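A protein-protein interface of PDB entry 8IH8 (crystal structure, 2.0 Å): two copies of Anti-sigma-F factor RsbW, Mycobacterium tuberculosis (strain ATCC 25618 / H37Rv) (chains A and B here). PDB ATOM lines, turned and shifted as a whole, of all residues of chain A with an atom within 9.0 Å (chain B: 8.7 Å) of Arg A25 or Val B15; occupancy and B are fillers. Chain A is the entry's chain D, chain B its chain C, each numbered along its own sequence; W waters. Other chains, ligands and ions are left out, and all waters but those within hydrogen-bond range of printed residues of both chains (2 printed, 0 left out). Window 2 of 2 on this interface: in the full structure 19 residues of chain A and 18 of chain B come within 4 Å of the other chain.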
ATOM      1  N   ASN A  21      19.347   5.183  11.384  1.00  0.00           N
ATOM      2  CA  ASN A  21      19.967   5.676  10.157  1.00  0.00           C
ATOM      3  C   ASN A  21      18.879   6.060   9.168  1.00  0.00           C
ATOM      4  O   ASN A  21      18.008   5.238   8.857  1.00  0.00           O
ATOM      5  CB  ASN A  21      20.872   4.610   9.524  1.00  0.00           C
ATOM      6  CG  ASN A  21      22.073   4.278  10.390  1.00  0.00           C
ATOM      7  OD1 ASN A  21      23.000   5.060  10.493  1.00  0.00           O
ATOM      8  ND2 ASN A  21      22.051   3.119  11.014  1.00  0.00           N
ATOM      9  N   VAL A  22      18.948   7.294   8.664  1.00  0.00           N
ATOM     10  CA  VAL A  22      18.049   7.806   7.634  1.00  0.00           C
ATOM     11  C   VAL A  22      18.875   8.581   6.612  1.00  0.00           C
ATOM     12  O   VAL A  22      19.974   9.052   6.898  1.00  0.00           O
ATOM     13  CB  VAL A  22      16.967   8.733   8.211  1.00  0.00           C
ATOM     14  CG1 VAL A  22      16.212   8.050   9.319  1.00  0.00           C
ATOM     15  CG2 VAL A  22      17.611  10.029   8.708  1.00  0.00           C
ATOM     16  N   ALA A  23      18.330   8.726   5.413  1.00  0.00           N
ATOM     17  CA  ALA A  23      19.006   9.543   4.418  1.00  0.00           C
ATOM     18  C   ALA A  23      19.197  10.948   4.985  1.00  0.00           C
ATOM     19  O   ALA A  23      18.287  11.507   5.604  1.00  0.00           O
ATOM     20  CB  ALA A  23      18.207   9.579   3.112  1.00  0.00           C
ATOM     21  N   ALA A  24      20.403  11.501   4.820  1.00  0.00           N
ATOM     22  CA  ALA A  24      20.718  12.834   5.361  1.00  0.00           C
ATOM     23  C   ALA A  24      20.055  13.892   4.495  1.00  0.00           C
ATOM     24  O   ALA A  24      20.676  14.506   3.620  1.00  0.00           O
ATOM     25  CB  ALA A  24      22.222  13.085   5.407  1.00  0.00           C
ATOM     26  N   ARG A  25      18.774  14.134   4.740  1.00  0.00           N
ATOM     27  CA  ARG A  25      18.159  15.185   3.958  1.00  0.00           C
ATOM     28  C   ARG A  25      17.058  15.926   4.669  1.00  0.00           C
ATOM     29  O   ARG A  25      16.431  15.415   5.595  1.00  0.00           O
ATOM     30  CB  ARG A  25      17.562  14.667   2.713  1.00  0.00           C
ATOM     31  CG  ARG A  25      18.473  13.949   1.922  1.00  0.00           C
ATOM     32  CD  ARG A  25      17.515  13.288   1.154  1.00  0.00           C
ATOM     33  NE  ARG A  25      18.060  13.173  -0.155  1.00  0.00           N
ATOM     34  CZ  ARG A  25      17.278  12.986  -1.192  1.00  0.00           C
ATOM     35  NH1 ARG A  25      15.970  12.966  -1.017  1.00  0.00           N
ATOM     36  NH2 ARG A  25      17.789  12.915  -2.395  1.00  0.00           N
ATOM     37  N   LEU A  26      16.789  17.123   4.125  1.00  0.00           N
ATOM     38  CA  LEU A  26      15.854  18.053   4.744  1.00  0.00           C
ATOM     39  C   LEU A  26      14.488  17.421   4.950  1.00  0.00           C
ATOM     40  O   LEU A  26      13.820  17.720   5.944  1.00  0.00           O
ATOM     41  CB  LEU A  26      15.748  19.321   3.896  1.00  0.00           C
ATOM     42  CG  LEU A  26      17.081  20.043   3.705  1.00  0.00           C
ATOM     43  CD1 LEU A  26      16.877  21.338   2.962  1.00  0.00           C
ATOM     44  CD2 LEU A  26      17.644  20.365   5.084  1.00  0.00           C
ATOM     45  N   GLU A  27      14.054  16.554   4.017  1.00  0.00           N
ATOM     46  CA  GLU A  27      12.751  15.890   4.125  1.00  0.00           C
ATOM     47  C   GLU A  27      12.642  14.979   5.340  1.00  0.00           C
ATOM     48  O   GLU A  27      11.525  14.583   5.710  1.00  0.00           O
ATOM     49  CB  GLU A  27      12.447  15.039   2.883  1.00  0.00           C
ATOM     50  CG  GLU A  27      12.153  15.836   1.623  1.00  0.00           C
ATOM     51  CD  GLU A  27      13.397  16.469   1.018  1.00  0.00           C
ATOM     52  OE1 GLU A  27      14.518  16.003   1.332  1.00  0.00           O
ATOM     53  OE2 GLU A  27      13.247  17.457   0.250  1.00  0.00           O
ATOM     54  N   ASN A  28      13.763  14.590   5.934  1.00  0.00           N
ATOM     55  CA  ASN A  28      13.752  13.701   7.083  1.00  0.00           C
ATOM     56  C   ASN A  28      13.958  14.448   8.379  1.00  0.00           C
ATOM     57  O   ASN A  28      14.080  13.828   9.440  1.00  0.00           O
ATOM     58  CB  ASN A  28      14.818  12.642   6.913  1.00  0.00           C
ATOM     59  CG  ASN A  28      14.446  11.685   5.821  1.00  0.00           C
ATOM     60  OD1 ASN A  28      13.265  11.621   5.481  1.00  0.00           O
ATOM     61  ND2 ASN A  28      15.419  10.988   5.222  1.00  0.00           N
ATOM     62  N   LEU A  29      14.028  15.768   8.309  1.00  0.00           N
ATOM     63  CA  LEU A  29      14.444  16.530   9.469  1.00  0.00           C
ATOM     64  C   LEU A  29      13.375  16.410  10.561  1.00  0.00           C
ATOM     65  O   LEU A  29      13.643  16.061  11.721  1.00  0.00           O
ATOM     66  CB  LEU A  29      14.705  17.975   9.012  1.00  0.00           C
ATOM     67  CG  LEU A  29      15.208  18.791  10.167  1.00  0.00           C
ATOM     68  CD1 LEU A  29      16.545  18.015  10.485  1.00  0.00           C
ATOM     69  CD2 LEU A  29      15.434  20.394   9.913  1.00  0.00           C
ATOM     70  N   ALA A  30      12.120  16.540  10.149  1.00  0.00           N
ATOM     71  CA  ALA A  30      10.985  16.444  11.068  1.00  0.00           C
ATOM     72  C   ALA A  30      10.773  15.017  11.566  1.00  0.00           C
ATOM     73  O   ALA A  30      10.320  14.807  12.699  1.00  0.00           O
ATOM     74  CB  ALA A  30       9.765  16.956  10.329  1.00  0.00           C
ATOM     75  N   LEU A  31      11.042  14.023  10.706  1.00  0.00           N
ATOM     76  CA  LEU A  31      10.979  12.632  11.137  1.00  0.00           C
ATOM     77  C   LEU A  31      11.950  12.380  12.282  1.00  0.00           C
ATOM     78  O   LEU A  31      11.599  11.751  13.288  1.00  0.00           O
ATOM     79  CB  LEU A  31      11.296  11.712   9.955  1.00  0.00           C
ATOM     80  CG  LEU A  31      11.523  10.212  10.221  1.00  0.00           C
ATOM     81  CD1 LEU A  31      10.293   9.524  10.835  1.00  0.00           C
ATOM     82  CD2 LEU A  31      11.926   9.554   8.913  1.00  0.00           C
ATOM     83  N   LEU A  32      13.183  12.860  12.142  1.00  0.00           N
ATOM     84  CA  LEU A  32      14.167  12.683  13.202  1.00  0.00           C
ATOM     85  C   LEU A  32      13.670  13.296  14.508  1.00  0.00           C
ATOM     86  O   LEU A  32      13.771  12.677  15.577  1.00  0.00           O
ATOM     87  CB  LEU A  32      15.492  13.296  12.759  1.00  0.00           C
ATOM     88  CG  LEU A  32      16.249  12.484  11.707  1.00  0.00           C
ATOM     89  CD1 LEU A  32      17.361  13.265  11.033  1.00  0.00           C
ATOM     90  CD2 LEU A  32      16.840  11.281  12.376  1.00  0.00           C
ATOM     91  N   CYS A  61      21.236  17.923  13.688  1.00  0.00           N
ATOM     92  CA  CYS A  61      20.813  17.267  12.458  1.00  0.00           C
ATOM     93  C   CYS A  61      20.642  18.268  11.320  1.00  0.00           C
ATOM     94  O   CYS A  61      20.982  17.975  10.166  1.00  0.00           O
ATOM     95  CB  CYS A  61      19.508  16.505  12.704  1.00  0.00           C
ATOM     96  SG  CYS A  61      19.746  15.039  13.736  1.00  0.00           S
ATOM     97  N   THR A  62      20.107  19.455  11.620  1.00  0.00           N
ATOM     98  CA  THR A  62      20.018  20.496  10.603  1.00  0.00           C
ATOM     99  C   THR A  62      21.397  20.839  10.055  1.00  0.00           C
ATOM    100  O   THR A  62      21.583  20.930   8.837  1.00  0.00           O
ATOM    101  CB  THR A  62      19.340  21.748  11.170  1.00  0.00           C
ATOM    102  OG1 THR A  62      18.009  21.412  11.574  1.00  0.00           O
ATOM    103  CG2 THR A  62      19.312  22.911  10.125  1.00  0.00           C
ATOM    104  N   LEU A  64      24.215  19.064  10.133  1.00  0.00           N
ATOM    105  CA  LEU A  64      24.747  17.931   9.380  1.00  0.00           C
ATOM    106  C   LEU A  64      24.096  17.851   8.013  1.00  0.00           C
ATOM    107  O   LEU A  64      24.766  17.757   6.977  1.00  0.00           O
ATOM    108  CB  LEU A  64      24.502  16.636  10.157  1.00  0.00           C
ATOM    109  CG  LEU A  64      25.405  16.467  11.369  1.00  0.00           C
ATOM    110  CD1 LEU A  64      24.943  15.278  12.255  1.00  0.00           C
ATOM    111  CD2 LEU A  64      26.854  16.281  10.911  1.00  0.00           C
ATOM    112  N   ILE A  65      22.773  17.869   7.993  1.00  0.00           N
ATOM    113  CA  ILE A  65      22.103  17.675   6.728  1.00  0.00           C
ATOM    114  C   ILE A  65      22.449  18.802   5.811  1.00  0.00           C
ATOM    115  O   ILE A  65      22.493  18.629   4.586  1.00  0.00           O
ATOM    116  CB  ILE A  65      20.596  17.567   6.939  1.00  0.00           C
ATOM    117  CG1 ILE A  65      20.296  16.155   7.435  1.00  0.00           C
ATOM    118  CG2 ILE A  65      19.842  17.882   5.630  1.00  0.00           C
ATOM    119  CD1 ILE A  65      18.894  15.999   8.007  1.00  0.00           C
ATOM    120  N   ARG A  66      22.754  19.966   6.354  1.00  0.00           N
ATOM    121  CA  ARG A  66      22.647  20.986   5.367  1.00  0.00           C
ATOM    122  C   ARG A  66      24.022  20.984   4.650  1.00  0.00           C
ATOM    123  O   ARG A  66      24.186  21.524   3.554  1.00  0.00           O
ATOM    124  CB  ARG A  66      22.383  22.364   6.031  1.00  0.00           C
ATOM    125  CG  ARG A  66      22.110  23.405   4.988  1.00  0.00           C
ATOM    126  CD  ARG A  66      21.781  24.898   5.453  1.00  0.00           C
ATOM    127  NE  ARG A  66      20.623  25.399   6.201  1.00  0.00           N
ATOM    128  CZ  ARG A  66      20.625  26.670   6.618  1.00  0.00           C
ATOM    129  NH1 ARG A  66      21.605  27.429   6.070  1.00  0.00           N
ATOM    130  NH2 ARG A  66      19.647  27.202   7.400  1.00  0.00           N
ATOM    131  N   SER A  67      25.050  20.342   5.262  1.00  0.00           N
ATOM    132  CA  SER A  67      26.374  20.080   4.663  1.00  0.00           C
ATOM    133  C   SER A  67      26.583  18.639   4.159  1.00  0.00           C
ATOM    134  O   SER A  67      27.694  18.304   3.685  1.00  0.00           O
ATOM    135  CB  SER A  67      27.526  20.359   5.658  1.00  0.00           C
ATOM    136  OG  SER A  67      27.644  21.723   6.027  1.00  0.00           O
ATOM    137  N   ALA A  68      25.591  17.770   4.264  1.00  0.00           N
ATOM    138  CA  ALA A  68      25.798  16.360   3.948  1.00  0.00           C
ATOM    139  C   ALA A  68      26.012  16.161   2.452  1.00  0.00           C
ATOM    140  O   ALA A  68      25.451  16.876   1.626  1.00  0.00           O
ATOM    141  CB  ALA A  68      24.592  15.525   4.415  1.00  0.00           C
ATOM    142  N   LEU A  69      26.825  15.160   2.102  1.00  0.00           N
ATOM    143  CA  LEU A  69      26.951  14.775   0.699  1.00  0.00           C
ATOM    144  C   LEU A  69      25.600  14.291   0.173  1.00  0.00           C
ATOM    145  O   LEU A  69      24.758  13.827   0.948  1.00  0.00           O
ATOM    146  CB  LEU A  69      27.992  13.665   0.533  1.00  0.00           C
ATOM    147  CG  LEU A  69      29.438  14.092   0.212  1.00  0.00           C
ATOM    148  CD1 LEU A  69      29.985  15.090   1.226  1.00  0.00           C
ATOM    149  CD2 LEU A  69      30.335  12.873   0.148  1.00  0.00           C
ATOM    150  N   PRO A  70      25.395  14.349  -1.152  1.00  0.00           N
ATOM    151  CA  PRO A  70      24.073  14.019  -1.730  1.00  0.00           C
ATOM    152  C   PRO A  70      23.512  12.665  -1.331  1.00  0.00           C
ATOM    153  O   PRO A  70      22.290  12.525  -1.187  1.00  0.00           O
ATOM    154  CB  PRO A  70      24.335  14.062  -3.244  1.00  0.00           C
ATOM    155  CG  PRO A  70      25.502  14.958  -3.399  1.00  0.00           C
ATOM    156  CD  PRO A  70      26.360  14.764  -2.179  1.00  0.00           C
ATOM    157  N   ASP A  71      24.337  11.643  -1.197  1.00  0.00           N
ATOM    158  CA  ASP A  71      23.780  10.330  -0.889  1.00  0.00           C
ATOM    159  C   ASP A  71      24.198   9.850   0.490  1.00  0.00           C
ATOM    160  O   ASP A  71      24.319   8.646   0.735  1.00  0.00           O
ATOM    161  CB  ASP A  71      24.148   9.324  -1.971  1.00  0.00           C
ATOM    162  CG  ASP A  71      23.587   9.720  -3.347  1.00  0.00           C
ATOM    163  OD1 ASP A  71      24.371  10.012  -4.282  1.00  0.00           O
ATOM    164  OD2 ASP A  71      22.340   9.733  -3.486  1.00  0.00           O
ATOM    165  N   ALA A  72      24.384  10.795   1.401  1.00  0.00           N
ATOM    166  CA  ALA A  72      24.872  10.496   2.733  1.00  0.00           C
ATOM    167  C   ALA A  72      23.755   9.994   3.636  1.00  0.00           C
ATOM    168  O   ALA A  72      22.589  10.371   3.498  1.00  0.00           O
ATOM    169  CB  ALA A  72      25.501  11.733   3.360  1.00  0.00           C
ATOM    170  N   THR A  73      24.143   9.153   4.586  1.00  0.00           N
ATOM    171  CA  THR A  73      23.267   8.679   5.650  1.00  0.00           C
ATOM    172  C   THR A  73      23.527   9.471   6.916  1.00  0.00           C
ATOM    173  O   THR A  73      24.686   9.667   7.304  1.00  0.00           O
ATOM    174  CB  THR A  73      23.522   7.197   5.899  1.00  0.00           C
ATOM    175  OG1 THR A  73      23.081   6.486   4.756  1.00  0.00           O
ATOM    176  CG2 THR A  73      22.785   6.702   7.140  1.00  0.00           C
ATOM    177  N   LEU A  74      22.459   9.940   7.558  1.00  0.00           N
ATOM    178  CA  LEU A  74      22.589  10.560   8.869  1.00  0.00           C
ATOM    179  C   LEU A  74      22.437   9.454   9.906  1.00  0.00           C
ATOM    180  O   LEU A  74      21.420   8.755   9.914  1.00  0.00           O
ATOM    181  CB  LEU A  74      21.554  11.663   9.068  1.00  0.00           C
ATOM    182  CG  LEU A  74      21.835  12.422  10.386  1.00  0.00           C
ATOM    183  CD1 LEU A  74      21.347  13.804  10.291  1.00  0.00           C
ATOM    184  CD2 LEU A  74      21.091  11.746  11.544  1.00  0.00           C
ATOM    185  N   ALA A  91      27.406  12.377   9.842  1.00  0.00           N
ATOM    186  CA  ALA A  91      27.092  12.221   8.431  1.00  0.00           C
ATOM    187  C   ALA A  91      28.339  12.555   7.628  1.00  0.00           C
ATOM    188  O   ALA A  91      29.165  13.358   8.068  1.00  0.00           O
ATOM    189  CB  ALA A  91      25.932  13.142   8.027  1.00  0.00           C
ATOM    190  N   GLN B  12      17.249  -0.405  -2.598  1.00  0.00           N
ATOM    191  CA  GLN B  12      15.908  -0.109  -3.090  1.00  0.00           C
ATOM    192  C   GLN B  12      15.244   1.041  -2.343  1.00  0.00           C
ATOM    193  O   GLN B  12      14.195   1.538  -2.756  1.00  0.00           O
ATOM    194  CB  GLN B  12      14.997  -1.326  -2.949  1.00  0.00           C
ATOM    195  CG  GLN B  12      15.643  -2.662  -3.177  1.00  0.00           C
ATOM    196  CD  GLN B  12      16.475  -2.699  -4.433  1.00  0.00           C
ATOM    197  OE1 GLN B  12      16.188  -1.996  -5.403  1.00  0.00           O
ATOM    198  NE2 GLN B  12      17.499  -3.546  -4.436  1.00  0.00           N
ATOM    199  N   ARG B  13      15.847   1.456  -1.235  1.00  0.00           N
ATOM    200  CA  ARG B  13      15.072   2.053  -0.158  1.00  0.00           C
ATOM    201  C   ARG B  13      14.584   3.453  -0.518  1.00  0.00           C
ATOM    202  O   ARG B  13      15.286   4.227  -1.175  1.00  0.00           O
ATOM    203  CB  ARG B  13      15.915   2.117   1.103  1.00  0.00           C
ATOM    204  CG  ARG B  13      16.062   0.782   1.777  1.00  0.00           C
ATOM    205  CD  ARG B  13      16.799   0.988   3.063  1.00  0.00           C
ATOM    206  NE  ARG B  13      17.412  -0.223   3.596  1.00  0.00           N
ATOM    207  CZ  ARG B  13      18.394  -0.193   4.491  1.00  0.00           C
ATOM    208  NH1 ARG B  13      18.829   0.978   4.953  1.00  0.00           N
ATOM    209  NH2 ARG B  13      18.924  -1.321   4.942  1.00  0.00           N
ATOM    210  N   GLY B  14      13.379   3.778  -0.069  1.00  0.00           N
ATOM    211  CA  GLY B  14      12.860   5.109  -0.276  1.00  0.00           C
ATOM    212  C   GLY B  14      13.559   6.127   0.605  1.00  0.00           C
ATOM    213  O   GLY B  14      14.277   5.812   1.557  1.00  0.00           O
ATOM    214  N   VAL B  15      13.302   7.395   0.294  1.00  0.00           N
ATOM    215  CA  VAL B  15      13.984   8.468   1.006  1.00  0.00           C
ATOM    216  C   VAL B  15      13.578   8.511   2.475  1.00  0.00           C
ATOM    217  O   VAL B  15      14.353   8.972   3.326  1.00  0.00           O
ATOM    218  CB  VAL B  15      13.724   9.810   0.287  1.00  0.00           C
ATOM    219  CG1 VAL B  15      12.248  10.185   0.347  1.00  0.00           C
ATOM    220  CG2 VAL B  15      14.601  10.918   0.874  1.00  0.00           C
ATOM    221  N   ARG B  16      12.394   8.012   2.815  1.00  0.00           N
ATOM    222  CA  ARG B  16      11.906   8.056   4.191  1.00  0.00           C
ATOM    223  C   ARG B  16      12.185   6.783   4.980  1.00  0.00           C
ATOM    224  O   ARG B  16      11.676   6.633   6.099  1.00  0.00           O
ATOM    225  CB  ARG B  16      10.409   8.341   4.220  1.00  0.00           C
ATOM    226  CG  ARG B  16      10.119   9.811   4.194  1.00  0.00           C
ATOM    227  CD  ARG B  16      10.338  10.428   5.580  1.00  0.00           C
ATOM    228  NE  ARG B  16      10.130  11.873   5.503  1.00  0.00           N
ATOM    229  CZ  ARG B  16       8.935  12.441   5.391  1.00  0.00           C
ATOM    230  NH1 ARG B  16       7.839  11.677   5.367  1.00  0.00           N
ATOM    231  NH2 ARG B  16       8.833  13.762   5.309  1.00  0.00           N
ATOM    232  N   ALA B  17      12.975   5.874   4.438  1.00  0.00           N
ATOM    233  CA  ALA B  17      13.274   4.637   5.139  1.00  0.00           C
ATOM    234  C   ALA B  17      14.085   4.916   6.400  1.00  0.00           C
ATOM    235  O   ALA B  17      14.967   5.785   6.421  1.00  0.00           O
ATOM    236  CB  ALA B  17      14.031   3.688   4.212  1.00  0.00           C
ATOM    237  N   VAL B  18      13.774   4.182   7.459  1.00  0.00           N
ATOM    238  CA  VAL B  18      14.455   4.314   8.744  1.00  0.00           C
ATOM    239  C   VAL B  18      15.044   2.965   9.102  1.00  0.00           C
ATOM    240  O   VAL B  18      14.318   1.962   9.156  1.00  0.00           O
ATOM    241  CB  VAL B  18      13.515   4.785   9.860  1.00  0.00           C
ATOM    242  CG1 VAL B  18      14.305   4.904  11.180  1.00  0.00           C
ATOM    243  CG2 VAL B  18      12.863   6.110   9.477  1.00  0.00           C
ATOM    244  N   GLU B  43       4.027   9.304   9.345  1.00  0.00           N
ATOM    245  CA  GLU B  43       3.668   9.021   7.965  1.00  0.00           C
ATOM    246  C   GLU B  43       2.165   9.076   7.725  1.00  0.00           C
ATOM    247  O   GLU B  43       1.708   8.675   6.652  1.00  0.00           O
ATOM    248  CB  GLU B  43       4.206   7.656   7.566  1.00  0.00           C
ATOM    249  CG  GLU B  43       5.709   7.647   7.340  1.00  0.00           C
ATOM    250  CD  GLU B  43       6.120   8.506   6.173  1.00  0.00           C
ATOM    251  OE1 GLU B  43       5.354   8.591   5.191  1.00  0.00           O
ATOM    252  OE2 GLU B  43       7.233   9.057   6.222  1.00  0.00           O
ATOM    253  N   VAL B  78      12.147   0.107   8.418  1.00  0.00           N
ATOM    254  CA  VAL B  78      10.774   0.512   8.153  1.00  0.00           C
ATOM    255  C   VAL B  78      10.835   1.492   6.993  1.00  0.00           C
ATOM    256  O   VAL B  78      11.413   2.582   7.119  1.00  0.00           O
ATOM    257  CB  VAL B  78      10.123   1.164   9.382  1.00  0.00           C
ATOM    258  CG1 VAL B  78       8.717   1.628   9.049  1.00  0.00           C
ATOM    259  CG2 VAL B  78      10.127   0.199  10.571  1.00  0.00           C
ATOM    260  N   ASP B  79      10.250   1.112   5.864  1.00  0.00           N
ATOM    261  CA  ASP B  79      10.384   1.899   4.642  1.00  0.00           C
ATOM    262  C   ASP B  79       8.994   2.312   4.189  1.00  0.00           C
ATOM    263  O   ASP B  79       8.345   1.594   3.407  1.00  0.00           O
ATOM    264  CB  ASP B  79      11.129   1.107   3.574  1.00  0.00           C
ATOM    265  CG  ASP B  79      11.404   1.918   2.343  1.00  0.00           C
ATOM    266  OD1 ASP B  79      11.041   3.113   2.335  1.00  0.00           O
ATOM    267  OD2 ASP B  79      12.006   1.376   1.396  1.00  0.00           O
ATOM    268  N   PRO B  80       8.485   3.473   4.675  1.00  0.00           N
ATOM    269  CA  PRO B  80       7.166   3.948   4.253  1.00  0.00           C
ATOM    270  C   PRO B  80       7.204   4.480   2.844  1.00  0.00           C
ATOM    271  O   PRO B  80       7.870   5.467   2.514  1.00  0.00           O
ATOM    272  CB  PRO B  80       6.828   5.055   5.263  1.00  0.00           C
ATOM    273  CG  PRO B  80       8.126   5.466   5.864  1.00  0.00           C
ATOM    274  CD  PRO B  80       9.194   4.465   5.506  1.00  0.00           C
ATOM    275  N   ARG B  81       6.449   3.800   2.015  1.00  0.00           N
ATOM    276  CA  ARG B  81       6.317   4.123   0.617  1.00  0.00           C
ATOM    277  C   ARG B  81       5.011   4.836   0.336  1.00  0.00           C
ATOM    278  O   ARG B  81       4.059   4.761   1.103  1.00  0.00           O
ATOM    279  CB  ARG B  81       6.366   2.852  -0.196  1.00  0.00           C
ATOM    280  CG  ARG B  81       7.614   2.117  -0.042  1.00  0.00           C
ATOM    281  CD  ARG B  81       8.733   2.860  -0.659  1.00  0.00           C
ATOM    282  NE  ARG B  81       9.804   1.951  -0.372  1.00  0.00           N
ATOM    283  CZ  ARG B  81      10.140   0.961  -1.198  1.00  0.00           C
ATOM    284  NH1 ARG B  81      11.140   0.150  -0.850  1.00  0.00           N
ATOM    285  NH2 ARG B  81       9.457   0.728  -2.317  1.00  0.00           N
ATOM    286  N   LYS B  82       4.995   5.511  -0.796  1.00  0.00           N
ATOM    287  CA  LYS B  82       3.836   5.948  -1.559  1.00  0.00           C
ATOM    288  C   LYS B  82       2.526   5.203  -1.270  1.00  0.00           C
ATOM    289  O   LYS B  82       1.538   5.840  -0.895  1.00  0.00           O
ATOM    290  CB  LYS B  82       4.333   5.839  -2.986  1.00  0.00           C
ATOM    291  CG  LYS B  82       4.661   4.393  -3.307  1.00  0.00           C
ATOM    292  CD  LYS B  82       5.163   4.274  -4.694  1.00  0.00           C
ATOM    293  CE  LYS B  82       6.594   4.859  -4.620  1.00  0.00           C
ATOM    294  NZ  LYS B  82       7.429   3.955  -3.730  1.00  0.00           N
HETATM  295  O   HOH W   1       9.192  16.811   6.348  1.00  0.00           O
HETATM  296  O   HOH W   2      15.989   7.320   4.667  1.00  0.00           O
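NE of Arg B16 is in hydrogen-bond range of OD1 of Asn A28.
NH2 of Arg B16 lies within hydrogen-bond range of O of Glu A27, at 2.8 Å.
The backbone carbonyl oxygen (O) of Val B15 sits at hydrogen-bond distance from the side-chain amide nitrogen (ND2) of Asn A28.
N of Val B18 sits at hydrogen-bond distance from O of Val B78, 2.9 Å away.
N of Leu A74 sits at hydrogen-bond distance from O of Val A22 (2.7 Å).
The side-chain carboxylate of Glu B43 lies within salt-bridge range of the guanidinium group of Arg B16, 2.8 Å away.
The side-chain amide nitrogen of Asn A28 is in hydrogen-bond range of the backbone carbonyl oxygen of Ala A23 (2.9 Å).
Among the printed residues, pairs that only touch across the chains: Arg A25 with Val B15, Leu A31 with Val B18, Asn A21 with Val B18, Leu A31 with Arg B16, Val A22 with Val B18, Val A22 with Ala B17, Ala A23 with Val B15 and Asn A21 with Ala B17.
Printed residues of chain B within 4 Å of Val A22: Ala B17 and Val B18.
Ala A23 touches just one residue of chain B: Val B15.
Of chain B, only Val B15 comes within 4 Å of Arg A25.
Printed residues of chain B within 4 Å of Leu A31: Arg B16 (3.8 Å) and Val B18 (3.6 Å).
Arg B13 touches none of the printed residues of chain A.
Val B15 touches three residues of chain A.
Of the printed residues of chain A, Ala B17 touches Asn A21 (3.9 Å) and Val A22 (3.9 Å).
The nearest residue of chain B that does not touch Arg A25 is Arg B16 (7.2 Å).
The nearest printed residue of chain A that does not touch Ala B17 is Ala A23 (4.6 Å).
Of the 26 printed residues of chain A, 7 touch a printed residue of chain B.
Hydrophobic or aromatic side chains of chain A within 4 Å of the printed part of chain B: Val A22, Ala A23 and Leu A31.
Of the 13 printed residues of chain B, 4 touch a printed residue of chain A.
Printed residues of chain B that touch a printed residue of chain A: Val B15, Arg B16, Ala B17 and Val B18.
Hydrophobic or aromatic side chains of chain B that line the printed part of chain A: Val B15 and Val B18.
No position is printed for both chains.
Water W2 lies within hydrogen-bond range of the backbone carbonyl oxygen of Ala B17 (2.5 Å), the backbone carbonyl oxygen of Val B15 (2.7 Å) and the backbone NH of Ala A23 (2.8 Å).
Water W1 bridges NH2 of Arg B16 and O of Glu A27.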
